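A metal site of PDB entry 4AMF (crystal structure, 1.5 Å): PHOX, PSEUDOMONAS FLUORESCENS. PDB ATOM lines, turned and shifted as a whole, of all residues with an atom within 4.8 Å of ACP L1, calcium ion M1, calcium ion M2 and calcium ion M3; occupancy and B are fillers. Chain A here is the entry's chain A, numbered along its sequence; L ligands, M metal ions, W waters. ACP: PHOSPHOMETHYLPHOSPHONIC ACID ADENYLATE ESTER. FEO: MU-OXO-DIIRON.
The side-chain carboxylate (OE1) of Glu 269 is bound to an iron atom (FE2) of FEO L2 (2.1 Å).
The side-chain carboxylate (OE2) of Glu 86 binds an iron atom (FE1) of FEO L2.
The side-chain carboxylate (OE2) of Glu 190 binds an iron atom (FE2) of FEO L2.
An oxygen (O2') of ACP L1 is in hydrogen-bond range of the side-chain amide oxygen (OD1) of Asn 191 (3.5 Å).
The guanidinium group (NH2) of Arg 290 is in hydrogen-bond range of an oxygen (O4') of ACP L1 (3.4 Å).
The side-chain carboxylate (OE2) of Glu 383 is bound to an iron atom (FE2) of FEO L2, at 2.1 Å.
The side-chain sulfur (SG) of Cys 175 is bound to an iron atom (FE1) of FEO L2 (2.6 Å).
The guanidinium group (NE) of Arg 381 is in hydrogen-bond range of an oxygen (O3') of ACP L1 (3.3 Å).
OD2 of Asp 288 is bound to FE2 of FEO L2 (2.1 Å).
An oxygen (O3G) of ACP L1 binds an iron atom (FE2) of FEO L2, 2.1 Å away.
The side-chain carboxylate (OD1) of Asp 288 is in salt-bridge range of the guanidinium group (NE) of Arg 381, at 2.8 Å.
O of Arg 381 lies within hydrogen-bond range of N of Thr 399, at 3.1 Å.
The side-chain carboxylate (OE1) of Glu 383 sits close to the side-chain hydroxyl (OG1) of Thr 399, 3.2 Å away.
The backbone carbonyl oxygen (O) of Asp 475 lies within hydrogen-bond range of the backbone NH (N) of Trp 384 (3.3 Å).
The side-chain carboxylate (OE2) of Glu 269 lies close to the indole nitrogen (NE1) of Trp 384 (3.2 Å).
The side-chain carboxylate of Glu 190 lies close to the side-chain amide nitrogen of Asn 191.
The side-chain carboxylate (OE1) of Glu 86 is in hydrogen-bond range of the side-chain amide nitrogen (NE2) of Gln 546 (3.3 Å).
The backbone carbonyl oxygen (O) of Glu 528 is in hydrogen-bond range of the backbone NH (N) of Gln 546, 3.0 Å away.
An oxygen (O2G) of ACP L1 sits close to the side-chain carboxylate of Glu 86.
O2G of ACP L1 sits close to OE1 of Glu 190 (2.9 Å).
The side-chain carboxylate of Asp 288 lies close to an oxygen (O3G) of ACP L1 (2.7 Å).
NE of Arg 219 touches C6 of ACP L1, at 3.4 Å.
Within 4 Å of ACP L1: Glu 86, Glu 190, Asn 191, Arg 219, Asp 288, Arg 290, Arg 381, Glu 383, Asp 475, Asp 490 and Glu 528.
Residues that only touch calcium ion M1: Arg 381.
The nearest printed residue that does not touch calcium ion M1 is Asp 288 (4.6 Å).
SG of Cys 175 touches calcium ion M2, 3.9 Å away.
Trp 384 touches calcium ion M2 (NE1 to CA, 3.9 Å).
Along chain A the residues within 4 Å of calcium ion M2 span positions 175 to 475.
Two residues have an atom within 4 Å of calcium ion M3: Asp 490 and Glu 528.
Calcium ion M1 is bound by water W9 (2.3 Å), the side-chain carboxylate (OD2) of Asp 475 (2.4 Å), the side-chain carboxylate (OD2) of Asp 490 (2.4 Å), an oxygen (O1G) of ACP L1 (2.4 Å), an oxygen (O1B) of ACP L1 (2.5 Å), the side-chain carboxylate (OE2) of Glu 383 (2.6 Å) and the side-chain carboxylate (OE1) of Glu 383 (2.7 Å).
Calcium ion M1 has seven donor atoms within binding distance.
Calcium ion M2 is bound by O of FEO L2 (2.2 Å).
OE2 of Glu 269 is bound to calcium ion M2.
Calcium ion M2 is bound by OD1 of Asp 475 (2.4 Å).
OD2 of Asp 475 binds calcium ion M2, 2.4 Å away.
Water W6 binds calcium ion M2 (2.5 Å).
Calcium ion M2 is bound by water W3 (2.6 Å).
Water W16 is bound to calcium ion M2, 2.7 Å away.
Calcium ion M2 has seven donor atoms within binding distance.
Slightly farther from calcium ion M2 lies OE2 of Glu 383 (2.9 Å).
Calcium ion M3 is bound by O1G of ACP L1 (2.3 Å), OE1 of Glu 528 (2.3 Å), OD2 of Asp 490 (2.3 Å), water W13 (2.4 Å), O2B of ACP L1 (2.5 Å), water W10 (2.5 Å) and OE2 of Glu 528 (2.8 Å).
Calcium ion M3 has seven donor atoms within binding distance.
Water W9 lies within hydrogen-bond range of the side-chain hydroxyl (OG1) of Thr 399 (2.8 Å) and the backbone carbonyl oxygen (O) of Asp 490 (2.9 Å).
Water W3 bridges the side-chain carboxylate of Asp 65 (2.6 Å) and the indole nitrogen of Trp 384 (2.9 Å).
Water W16 lies within hydrogen-bond range of the side-chain carboxylate (OD2) of Asp 65 (2.6 Å) and the side-chain carboxylate (OE1) of Glu 86 (3.1 Å).
Water W13 lies within hydrogen-bond range of OE1 of Glu 86 (2.6 Å) and OE1 of Gln 546 (2.8 Å).
Water W5 lies within hydrogen-bond range of an oxygen (O3') of ACP L1 (2.8 Å) and the backbone NH (N) of Arg 290 (2.9 Å).
Water W14 lies within hydrogen-bond range of the side-chain amide oxygen (OD1) of Asn 191, the backbone carbonyl oxygen (O) of Asp 288 and an oxygen (O2') of ACP L1.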
ATOM      1  N   ASP A  65     -36.962   9.099 -22.305  1.00  0.00           N
ATOM      2  CA  ASP A  65     -36.490   8.932 -23.679  1.00  0.00           C
ATOM      3  C   ASP A  65     -37.647   9.123 -24.671  1.00  0.00           C
ATOM      4  O   ASP A  65     -38.298  10.147 -24.597  1.00  0.00           O
ATOM      5  CB  ASP A  65     -35.741   7.587 -23.735  1.00  0.00           C
ATOM      6  CG  ASP A  65     -34.756   7.370 -24.840  1.00  0.00           C
ATOM      7  OD1 ASP A  65     -34.833   8.068 -25.847  1.00  0.00           O
ATOM      8  OD2 ASP A  65     -33.835   6.542 -24.646  1.00  0.00           O
ATOM      9  N   GLU A  86     -35.659   4.809 -19.926  1.00  0.00           N
ATOM     10  CA  GLU A  86     -34.735   3.826 -20.507  1.00  0.00           C
ATOM     11  C   GLU A  86     -33.830   3.101 -19.555  1.00  0.00           C
ATOM     12  O   GLU A  86     -33.652   1.882 -19.691  1.00  0.00           O
ATOM     13  CB  GLU A  86     -33.915   4.508 -21.637  1.00  0.00           C
ATOM     14  CG  GLU A  86     -33.136   3.481 -22.464  1.00  0.00           C
ATOM     15  CD  GLU A  86     -32.184   4.022 -23.498  1.00  0.00           C
ATOM     16  OE1 GLU A  86     -31.508   5.033 -23.210  1.00  0.00           O
ATOM     17  OE2 GLU A  86     -32.210   3.516 -24.629  1.00  0.00           O
ATOM     18  N   CYS A 175     -36.396   2.368 -24.962  1.00  0.00           N
ATOM     19  CA  CYS A 175     -35.651   3.376 -25.668  1.00  0.00           C
ATOM     20  C   CYS A 175     -36.570   4.364 -26.333  1.00  0.00           C
ATOM     21  O   CYS A 175     -37.010   5.366 -25.722  1.00  0.00           O
ATOM     22  CB  CYS A 175     -34.717   2.676 -26.637  1.00  0.00           C
ATOM     23  SG  CYS A 175     -33.780   3.768 -27.681  1.00  0.00           S
ATOM     24  N   GLU A 190     -34.547  -1.979 -26.149  1.00  0.00           N
ATOM     25  CA  GLU A 190     -33.294  -1.858 -26.882  1.00  0.00           C
ATOM     26  C   GLU A 190     -32.174  -2.638 -26.214  1.00  0.00           C
ATOM     27  O   GLU A 190     -32.018  -3.843 -26.491  1.00  0.00           O
ATOM     28  CB  GLU A 190     -32.945  -0.395 -27.093  1.00  0.00           C
ATOM     29  CG  GLU A 190     -31.727  -0.164 -27.970  1.00  0.00           C
ATOM     30  CD  GLU A 190     -31.162   1.230 -27.833  1.00  0.00           C
ATOM     31  OE1 GLU A 190     -31.363   1.853 -26.760  1.00  0.00           O
ATOM     32  OE2 GLU A 190     -30.564   1.737 -28.809  1.00  0.00           O
ATOM     33  N   ASN A 191     -31.380  -2.032 -25.315  1.00  0.00           N
ATOM     34  CA  ASN A 191     -30.216  -2.726 -24.736  1.00  0.00           C
ATOM     35  C   ASN A 191     -30.578  -3.635 -23.555  1.00  0.00           C
ATOM     36  O   ASN A 191     -29.924  -3.627 -22.516  1.00  0.00           O
ATOM     37  CB  ASN A 191     -29.126  -1.716 -24.397  1.00  0.00           C
ATOM     38  CG  ASN A 191     -28.493  -1.181 -25.676  1.00  0.00           C
ATOM     39  OD1 ASN A 191     -28.051  -1.964 -26.516  1.00  0.00           O
ATOM     40  ND2 ASN A 191     -28.534   0.127 -25.902  1.00  0.00           N
ATOM     41  N   ARG A 219     -23.580  -5.983 -18.421  1.00  0.00           N
ATOM     42  CA  ARG A 219     -22.901  -4.791 -18.885  1.00  0.00           C
ATOM     43  C   ARG A 219     -23.023  -3.722 -17.810  1.00  0.00           C
ATOM     44  O   ARG A 219     -23.740  -2.723 -17.985  1.00  0.00           O
ATOM     45  CB  ARG A 219     -23.432  -4.325 -20.254  1.00  0.00           C
ATOM     46  CG  ARG A 219     -22.513  -3.296 -20.927  1.00  0.00           C
ATOM     47  CD  ARG A 219     -22.888  -3.072 -22.360  1.00  0.00           C
ATOM     48  NE  ARG A 219     -22.617  -4.241 -23.195  1.00  0.00           N
ATOM     49  CZ  ARG A 219     -23.092  -4.432 -24.425  1.00  0.00           C
ATOM     50  NH1 ARG A 219     -23.884  -3.531 -24.992  1.00  0.00           N
ATOM     51  NH2 ARG A 219     -22.801  -5.538 -25.092  1.00  0.00           N
ATOM     52  N   GLU A 269     -34.960   0.303 -31.377  1.00  0.00           N
ATOM     53  CA  GLU A 269     -34.872   1.714 -31.032  1.00  0.00           C
ATOM     54  C   GLU A 269     -36.267   2.357 -31.034  1.00  0.00           C
ATOM     55  O   GLU A 269     -36.765   2.689 -29.984  1.00  0.00           O
ATOM     56  CB  GLU A 269     -33.944   2.477 -31.975  1.00  0.00           C
ATOM     57  CG  GLU A 269     -33.798   3.945 -31.590  1.00  0.00           C
ATOM     58  CD  GLU A 269     -32.562   4.307 -30.831  1.00  0.00           C
ATOM     59  OE1 GLU A 269     -31.647   3.467 -30.740  1.00  0.00           O
ATOM     60  OE2 GLU A 269     -32.551   5.426 -30.257  1.00  0.00           O
ATOM     61  N   ASP A 288     -30.476  -1.150 -32.913  1.00  0.00           N
ATOM     62  CA  ASP A 288     -29.352  -0.283 -32.633  1.00  0.00           C
ATOM     63  C   ASP A 288     -28.142  -0.991 -32.048  1.00  0.00           C
ATOM     64  O   ASP A 288     -27.890  -1.009 -30.845  1.00  0.00           O
ATOM     65  CB  ASP A 288     -29.733   0.916 -31.803  1.00  0.00           C
ATOM     66  CG  ASP A 288     -28.550   1.855 -31.626  1.00  0.00           C
ATOM     67  OD1 ASP A 288     -27.564   1.704 -32.370  1.00  0.00           O
ATOM     68  OD2 ASP A 288     -28.587   2.687 -30.741  1.00  0.00           O
ATOM     69  N   GLU A 289     -27.356  -1.482 -32.952  1.00  0.00           N
ATOM     70  CA  GLU A 289     -26.053  -2.088 -32.637  1.00  0.00           C
ATOM     71  C   GLU A 289     -25.151  -1.966 -33.872  1.00  0.00           C
ATOM     72  O   GLU A 289     -25.609  -2.133 -35.000  1.00  0.00           O
ATOM     73  CB  GLU A 289     -26.173  -3.527 -32.140  1.00  0.00           C
ATOM     74  CG  GLU A 289     -24.842  -4.111 -31.678  1.00  0.00           C
ATOM     75  CD  GLU A 289     -24.947  -5.424 -30.943  1.00  0.00           C
ATOM     76  OE1 GLU A 289     -26.016  -5.676 -30.331  1.00  0.00           O
ATOM     77  OE2 GLU A 289     -23.963  -6.202 -30.954  1.00  0.00           O
ATOM     78  N   ARG A 290     -23.890  -1.617 -33.662  1.00  0.00           N
ATOM     79  CA  ARG A 290     -22.964  -1.535 -34.793  1.00  0.00           C
ATOM     80  C   ARG A 290     -23.061  -2.784 -35.702  1.00  0.00           C
ATOM     81  O   ARG A 290     -22.941  -3.916 -35.234  1.00  0.00           O
ATOM     82  CB  ARG A 290     -21.508  -1.431 -34.309  1.00  0.00           C
ATOM     83  CG  ARG A 290     -21.108  -0.098 -33.711  1.00  0.00           C
ATOM     84  CD  ARG A 290     -19.638  -0.116 -33.336  1.00  0.00           C
ATOM     85  NE  ARG A 290     -19.410  -0.785 -32.067  1.00  0.00           N
ATOM     86  CZ  ARG A 290     -19.458  -0.194 -30.875  1.00  0.00           C
ATOM     87  NH1 ARG A 290     -19.730   1.112 -30.769  1.00  0.00           N
ATOM     88  NH2 ARG A 290     -19.245  -0.882 -29.773  1.00  0.00           N
ATOM     89  N   ARG A 381     -25.427   1.547 -36.987  1.00  0.00           N
ATOM     90  CA  ARG A 381     -26.283   1.831 -35.836  1.00  0.00           C
ATOM     91  C   ARG A 381     -27.568   2.592 -36.124  1.00  0.00           C
ATOM     92  O   ARG A 381     -27.686   3.784 -35.836  1.00  0.00           O
ATOM     93  CB  ARG A 381     -25.493   2.566 -34.763  1.00  0.00           C
ATOM     94  CG  ARG A 381     -24.437   1.702 -34.095  1.00  0.00           C
ATOM     95  CD  ARG A 381     -23.870   2.442 -32.931  1.00  0.00           C
ATOM     96  NE  ARG A 381     -24.917   2.663 -31.932  1.00  0.00           N
ATOM     97  CZ  ARG A 381     -24.867   3.557 -30.949  1.00  0.00           C
ATOM     98  NH1 ARG A 381     -23.783   4.309 -30.777  1.00  0.00           N
ATOM     99  NH2 ARG A 381     -25.891   3.697 -30.119  1.00  0.00           N
ATOM    100  N   GLU A 383     -30.823   4.225 -35.434  1.00  0.00           N
ATOM    101  CA  GLU A 383     -31.554   4.670 -34.266  1.00  0.00           C
ATOM    102  C   GLU A 383     -32.971   5.061 -34.726  1.00  0.00           C
ATOM    103  O   GLU A 383     -33.650   4.176 -35.257  1.00  0.00           O
ATOM    104  CB  GLU A 383     -30.777   5.679 -33.417  1.00  0.00           C
ATOM    105  CG  GLU A 383     -29.599   5.005 -32.720  1.00  0.00           C
ATOM    106  CD  GLU A 383     -29.060   5.724 -31.495  1.00  0.00           C
ATOM    107  OE1 GLU A 383     -28.292   6.687 -31.700  1.00  0.00           O
ATOM    108  OE2 GLU A 383     -29.443   5.412 -30.344  1.00  0.00           O
ATOM    109  N   TRP A 384     -33.452   6.276 -34.527  1.00  0.00           N
ATOM    110  CA  TRP A 384     -34.847   6.564 -34.825  1.00  0.00           C
ATOM    111  C   TRP A 384     -35.128   6.603 -36.305  1.00  0.00           C
ATOM    112  O   TRP A 384     -34.336   7.135 -37.089  1.00  0.00           O
ATOM    113  CB  TRP A 384     -35.315   7.874 -34.200  1.00  0.00           C
ATOM    114  CG  TRP A 384     -35.383   7.878 -32.716  1.00  0.00           C
ATOM    115  CD1 TRP A 384     -34.426   7.446 -31.858  1.00  0.00           C
ATOM    116  CD2 TRP A 384     -36.296   8.655 -31.930  1.00  0.00           C
ATOM    117  NE1 TRP A 384     -34.745   7.786 -30.575  1.00  0.00           N
ATOM    118  CE2 TRP A 384     -35.825   8.619 -30.589  1.00  0.00           C
ATOM    119  CE3 TRP A 384     -37.462   9.385 -32.218  1.00  0.00           C
ATOM    120  CZ2 TRP A 384     -36.479   9.274 -29.563  1.00  0.00           C
ATOM    121  CZ3 TRP A 384     -38.027  10.129 -31.208  1.00  0.00           C
ATOM    122  CH2 TRP A 384     -37.584  10.016 -29.888  1.00  0.00           C
ATOM    123  N   THR A 399     -26.310   6.515 -36.289  1.00  0.00           N
ATOM    124  CA  THR A 399     -25.671   7.403 -35.308  1.00  0.00           C
ATOM    125  C   THR A 399     -24.179   7.483 -35.349  1.00  0.00           C
ATOM    126  O   THR A 399     -23.632   8.583 -35.232  1.00  0.00           O
ATOM    127  CB  THR A 399     -26.223   7.182 -33.903  1.00  0.00           C
ATOM    128  OG1 THR A 399     -25.986   8.377 -33.128  1.00  0.00           O
ATOM    129  CG2 THR A 399     -25.679   5.974 -33.254  1.00  0.00           C
ATOM    130  N   ASP A 475     -29.584  10.896 -33.273  1.00  0.00           N
ATOM    131  CA  ASP A 475     -30.213   9.746 -32.645  1.00  0.00           C
ATOM    132  C   ASP A 475     -31.705   9.894 -32.862  1.00  0.00           C
ATOM    133  O   ASP A 475     -32.251   9.275 -33.800  1.00  0.00           O
ATOM    134  CB  ASP A 475     -29.719   9.679 -31.204  1.00  0.00           C
ATOM    135  CG  ASP A 475     -30.322   8.585 -30.347  1.00  0.00           C
ATOM    136  OD1 ASP A 475     -31.433   8.149 -30.644  1.00  0.00           O
ATOM    137  OD2 ASP A 475     -29.656   8.161 -29.377  1.00  0.00           O
ATOM    138  N   ASP A 490     -27.281  12.619 -29.579  1.00  0.00           N
ATOM    139  CA  ASP A 490     -26.736  11.833 -28.506  1.00  0.00           C
ATOM    140  C   ASP A 490     -25.310  11.502 -28.854  1.00  0.00           C
ATOM    141  O   ASP A 490     -24.961  10.347 -29.086  1.00  0.00           O
ATOM    142  CB  ASP A 490     -27.554  10.543 -28.289  1.00  0.00           C
ATOM    143  CG  ASP A 490     -26.934   9.614 -27.261  1.00  0.00           C
ATOM    144  OD1 ASP A 490     -26.206  10.106 -26.359  1.00  0.00           O
ATOM    145  OD2 ASP A 490     -27.172   8.381 -27.355  1.00  0.00           O
ATOM    146  N   GLU A 528     -28.078  13.879 -23.053  1.00  0.00           N
ATOM    147  CA  GLU A 528     -28.433  13.713 -24.433  1.00  0.00           C
ATOM    148  C   GLU A 528     -29.845  14.324 -24.582  1.00  0.00           C
ATOM    149  O   GLU A 528     -30.583  14.413 -23.584  1.00  0.00           O
ATOM    150  CB  GLU A 528     -28.336  12.302 -24.974  1.00  0.00           C
ATOM    151  CG  GLU A 528     -29.356  11.326 -24.433  1.00  0.00           C
ATOM    152  CD  GLU A 528     -29.013   9.913 -24.832  1.00  0.00           C
ATOM    153  OE1 GLU A 528     -28.073   9.365 -24.218  1.00  0.00           O
ATOM    154  OE2 GLU A 528     -29.626   9.378 -25.787  1.00  0.00           O
ATOM    155  N   THR A 530     -33.354  13.774 -26.187  1.00  0.00           N
ATOM    156  CA  THR A 530     -34.102  12.612 -26.708  1.00  0.00           C
ATOM    157  C   THR A 530     -35.572  12.709 -26.334  1.00  0.00           C
ATOM    158  O   THR A 530     -35.911  13.298 -25.308  1.00  0.00           O
ATOM    159  CB  THR A 530     -33.418  11.302 -26.256  1.00  0.00           C
ATOM    160  OG1 THR A 530     -34.066  10.204 -26.885  1.00  0.00           O
ATOM    161  CG2 THR A 530     -33.401  11.121 -24.765  1.00  0.00           C
ATOM    162  N   GLN A 546     -32.091  13.763 -21.086  1.00  0.00           N
ATOM    163  CA  GLN A 546     -31.771  12.486 -20.470  1.00  0.00           C
ATOM    164  C   GLN A 546     -30.392  12.488 -19.848  1.00  0.00           C
ATOM    165  O   GLN A 546     -29.436  12.986 -20.445  1.00  0.00           O
ATOM    166  CB  GLN A 546     -31.905  11.373 -21.511  1.00  0.00           C
ATOM    167  CG  GLN A 546     -31.993   9.984 -20.933  1.00  0.00           C
ATOM    168  CD  GLN A 546     -31.719   8.893 -21.942  1.00  0.00           C
ATOM    169  OE1 GLN A 546     -30.738   8.954 -22.674  1.00  0.00           O
ATOM    170  NE2 GLN A 546     -32.583   7.878 -22.017  1.00  0.00           N
ATOM    171  N   HIS A 547     -30.292  11.924 -18.659  1.00  0.00           N
ATOM    172  CA  HIS A 547     -29.088  11.808 -17.863  1.00  0.00           C
ATOM    173  C   HIS A 547     -28.215  13.070 -17.800  1.00  0.00           C
ATOM    174  O   HIS A 547     -27.008  12.995 -17.984  1.00  0.00           O
ATOM    175  CB  HIS A 547     -28.268  10.577 -18.283  1.00  0.00           C
ATOM    176  CG  HIS A 547     -27.768  10.579 -19.703  1.00  0.00           C
ATOM    177  ND1 HIS A 547     -26.753  11.414 -20.112  1.00  0.00           N
ATOM    178  CD2 HIS A 547     -28.171   9.847 -20.760  1.00  0.00           C
ATOM    179  CE1 HIS A 547     -26.546  11.163 -21.391  1.00  0.00           C
ATOM    180  NE2 HIS A 547     -27.380  10.221 -21.838  1.00  0.00           N
HETATM  181  PG  ACP L   1     -28.340   4.426 -26.902  1.00  0.00           P
HETATM  182  O1G ACP L   1     -28.552   5.999 -27.030  1.00  0.00           O
HETATM  183  O2G ACP L   1     -29.476   3.833 -25.870  1.00  0.00           O
HETATM  184  O3G ACP L   1     -28.337   3.740 -28.307  1.00  0.00           O
HETATM  185  PB  ACP L   1     -25.554   5.267 -26.800  1.00  0.00           P
HETATM  186  O1B ACP L   1     -25.736   5.601 -28.228  1.00  0.00           O
HETATM  187  O2B ACP L   1     -25.496   6.383 -25.732  1.00  0.00           O
HETATM  188  C3B ACP L   1     -26.717   4.073 -26.275  1.00  0.00           C
HETATM  189  PA  ACP L   1     -22.898   4.442 -25.939  1.00  0.00           P
HETATM  190  O1A ACP L   1     -23.270   4.111 -24.552  1.00  0.00           O
HETATM  191  O2A ACP L   1     -21.928   5.528 -26.261  1.00  0.00           O
HETATM  192  O3A ACP L   1     -24.147   4.570 -26.852  1.00  0.00           O
HETATM  193  O5' ACP L   1     -22.151   3.119 -26.608  1.00  0.00           O
HETATM  194  C5' ACP L   1     -21.964   3.003 -28.027  1.00  0.00           C
HETATM  195  C4' ACP L   1     -22.556   1.716 -28.546  1.00  0.00           C
HETATM  196  O4' ACP L   1     -21.760   0.615 -28.069  1.00  0.00           O
HETATM  197  C3' ACP L   1     -23.999   1.374 -28.184  1.00  0.00           C
HETATM  198  O3' ACP L   1     -24.641   0.736 -29.296  1.00  0.00           O
HETATM  199  C2' ACP L   1     -23.840   0.470 -26.962  1.00  0.00           C
HETATM  200  O2' ACP L   1     -24.961  -0.390 -26.817  1.00  0.00           O
HETATM  201  C1' ACP L   1     -22.541  -0.283 -27.298  1.00  0.00           C
HETATM  202  N9  ACP L   1     -21.755  -0.697 -26.151  1.00  0.00           N
HETATM  203  C8  ACP L   1     -21.577  -0.032 -24.968  1.00  0.00           C
HETATM  204  N7  ACP L   1     -20.795  -0.656 -24.110  1.00  0.00           N
HETATM  205  C5  ACP L   1     -20.432  -1.811 -24.779  1.00  0.00           C
HETATM  206  C6  ACP L   1     -19.659  -2.931 -24.391  1.00  0.00           C
HETATM  207  N6  ACP L   1     -19.160  -3.103 -23.172  1.00  0.00           N
HETATM  208  N1  ACP L   1     -19.497  -3.917 -25.306  1.00  0.00           N
HETATM  209  C2  ACP L   1     -20.089  -3.807 -26.496  1.00  0.00           C
HETATM  210  N3  ACP L   1     -20.853  -2.804 -26.955  1.00  0.00           N
HETATM  211  C4  ACP L   1     -21.000  -1.843 -26.049  1.00  0.00           C
HETATM  212 FE1  FEO L   2     -31.506   3.934 -26.480  1.00  0.00          FE
HETATM  213 FE2  FEO L   2     -30.009   3.580 -29.485  1.00  0.00          FE
HETATM  214  O   FEO L   2     -30.946   4.680 -28.166  1.00  0.00           O
HETATM  215 CA    CA M   1     -27.704   6.846 -29.113  1.00  0.00          CA
HETATM  216 CA    CA M   2     -31.489   6.768 -28.722  1.00  0.00          CA
HETATM  217 CA    CA M   3     -27.752   7.353 -25.325  1.00  0.00          CA
HETATM  218  O   HOH W   1     -27.334   1.089 -28.669  1.00  0.00           O
HETATM  219  O   HOH W   2     -23.893   8.491 -25.859  1.00  0.00           O
HETATM  220  O   HOH W   3     -33.975   6.862 -27.958  1.00  0.00           O
HETATM  221  O   HOH W   4     -21.657   7.389 -24.140  1.00  0.00           O
HETATM  222  O   HOH W   5     -23.139  -0.924 -30.988  1.00  0.00           O
HETATM  223  O   HOH W   6     -31.685   8.909 -27.521  1.00  0.00           O
HETATM  224  O   HOH W   7     -23.317   6.945 -29.648  1.00  0.00           O
HETATM  225  O   HOH W   8     -24.942   4.677 -22.748  1.00  0.00           O
HETATM  226  O   HOH W   9     -26.134   7.993 -30.358  1.00  0.00           O
HETATM  227  O   HOH W  10     -26.824   6.621 -23.117  1.00  0.00           O
HETATM  228  O   HOH W  11     -25.058  -1.123 -24.005  1.00  0.00           O
HETATM  229  O   HOH W  12     -22.097  -3.044 -29.500  1.00  0.00           O
HETATM  230  O   HOH W  13     -29.821   6.762 -24.194  1.00  0.00           O
HETATM  231  O   HOH W  14     -26.436  -2.095 -28.695  1.00  0.00           O
HETATM  232  O   HOH W  15     -29.127   2.074 -23.907  1.00  0.00           O
HETATM  233  O   HOH W  16     -31.730   6.229 -26.112  1.00  0.00           O
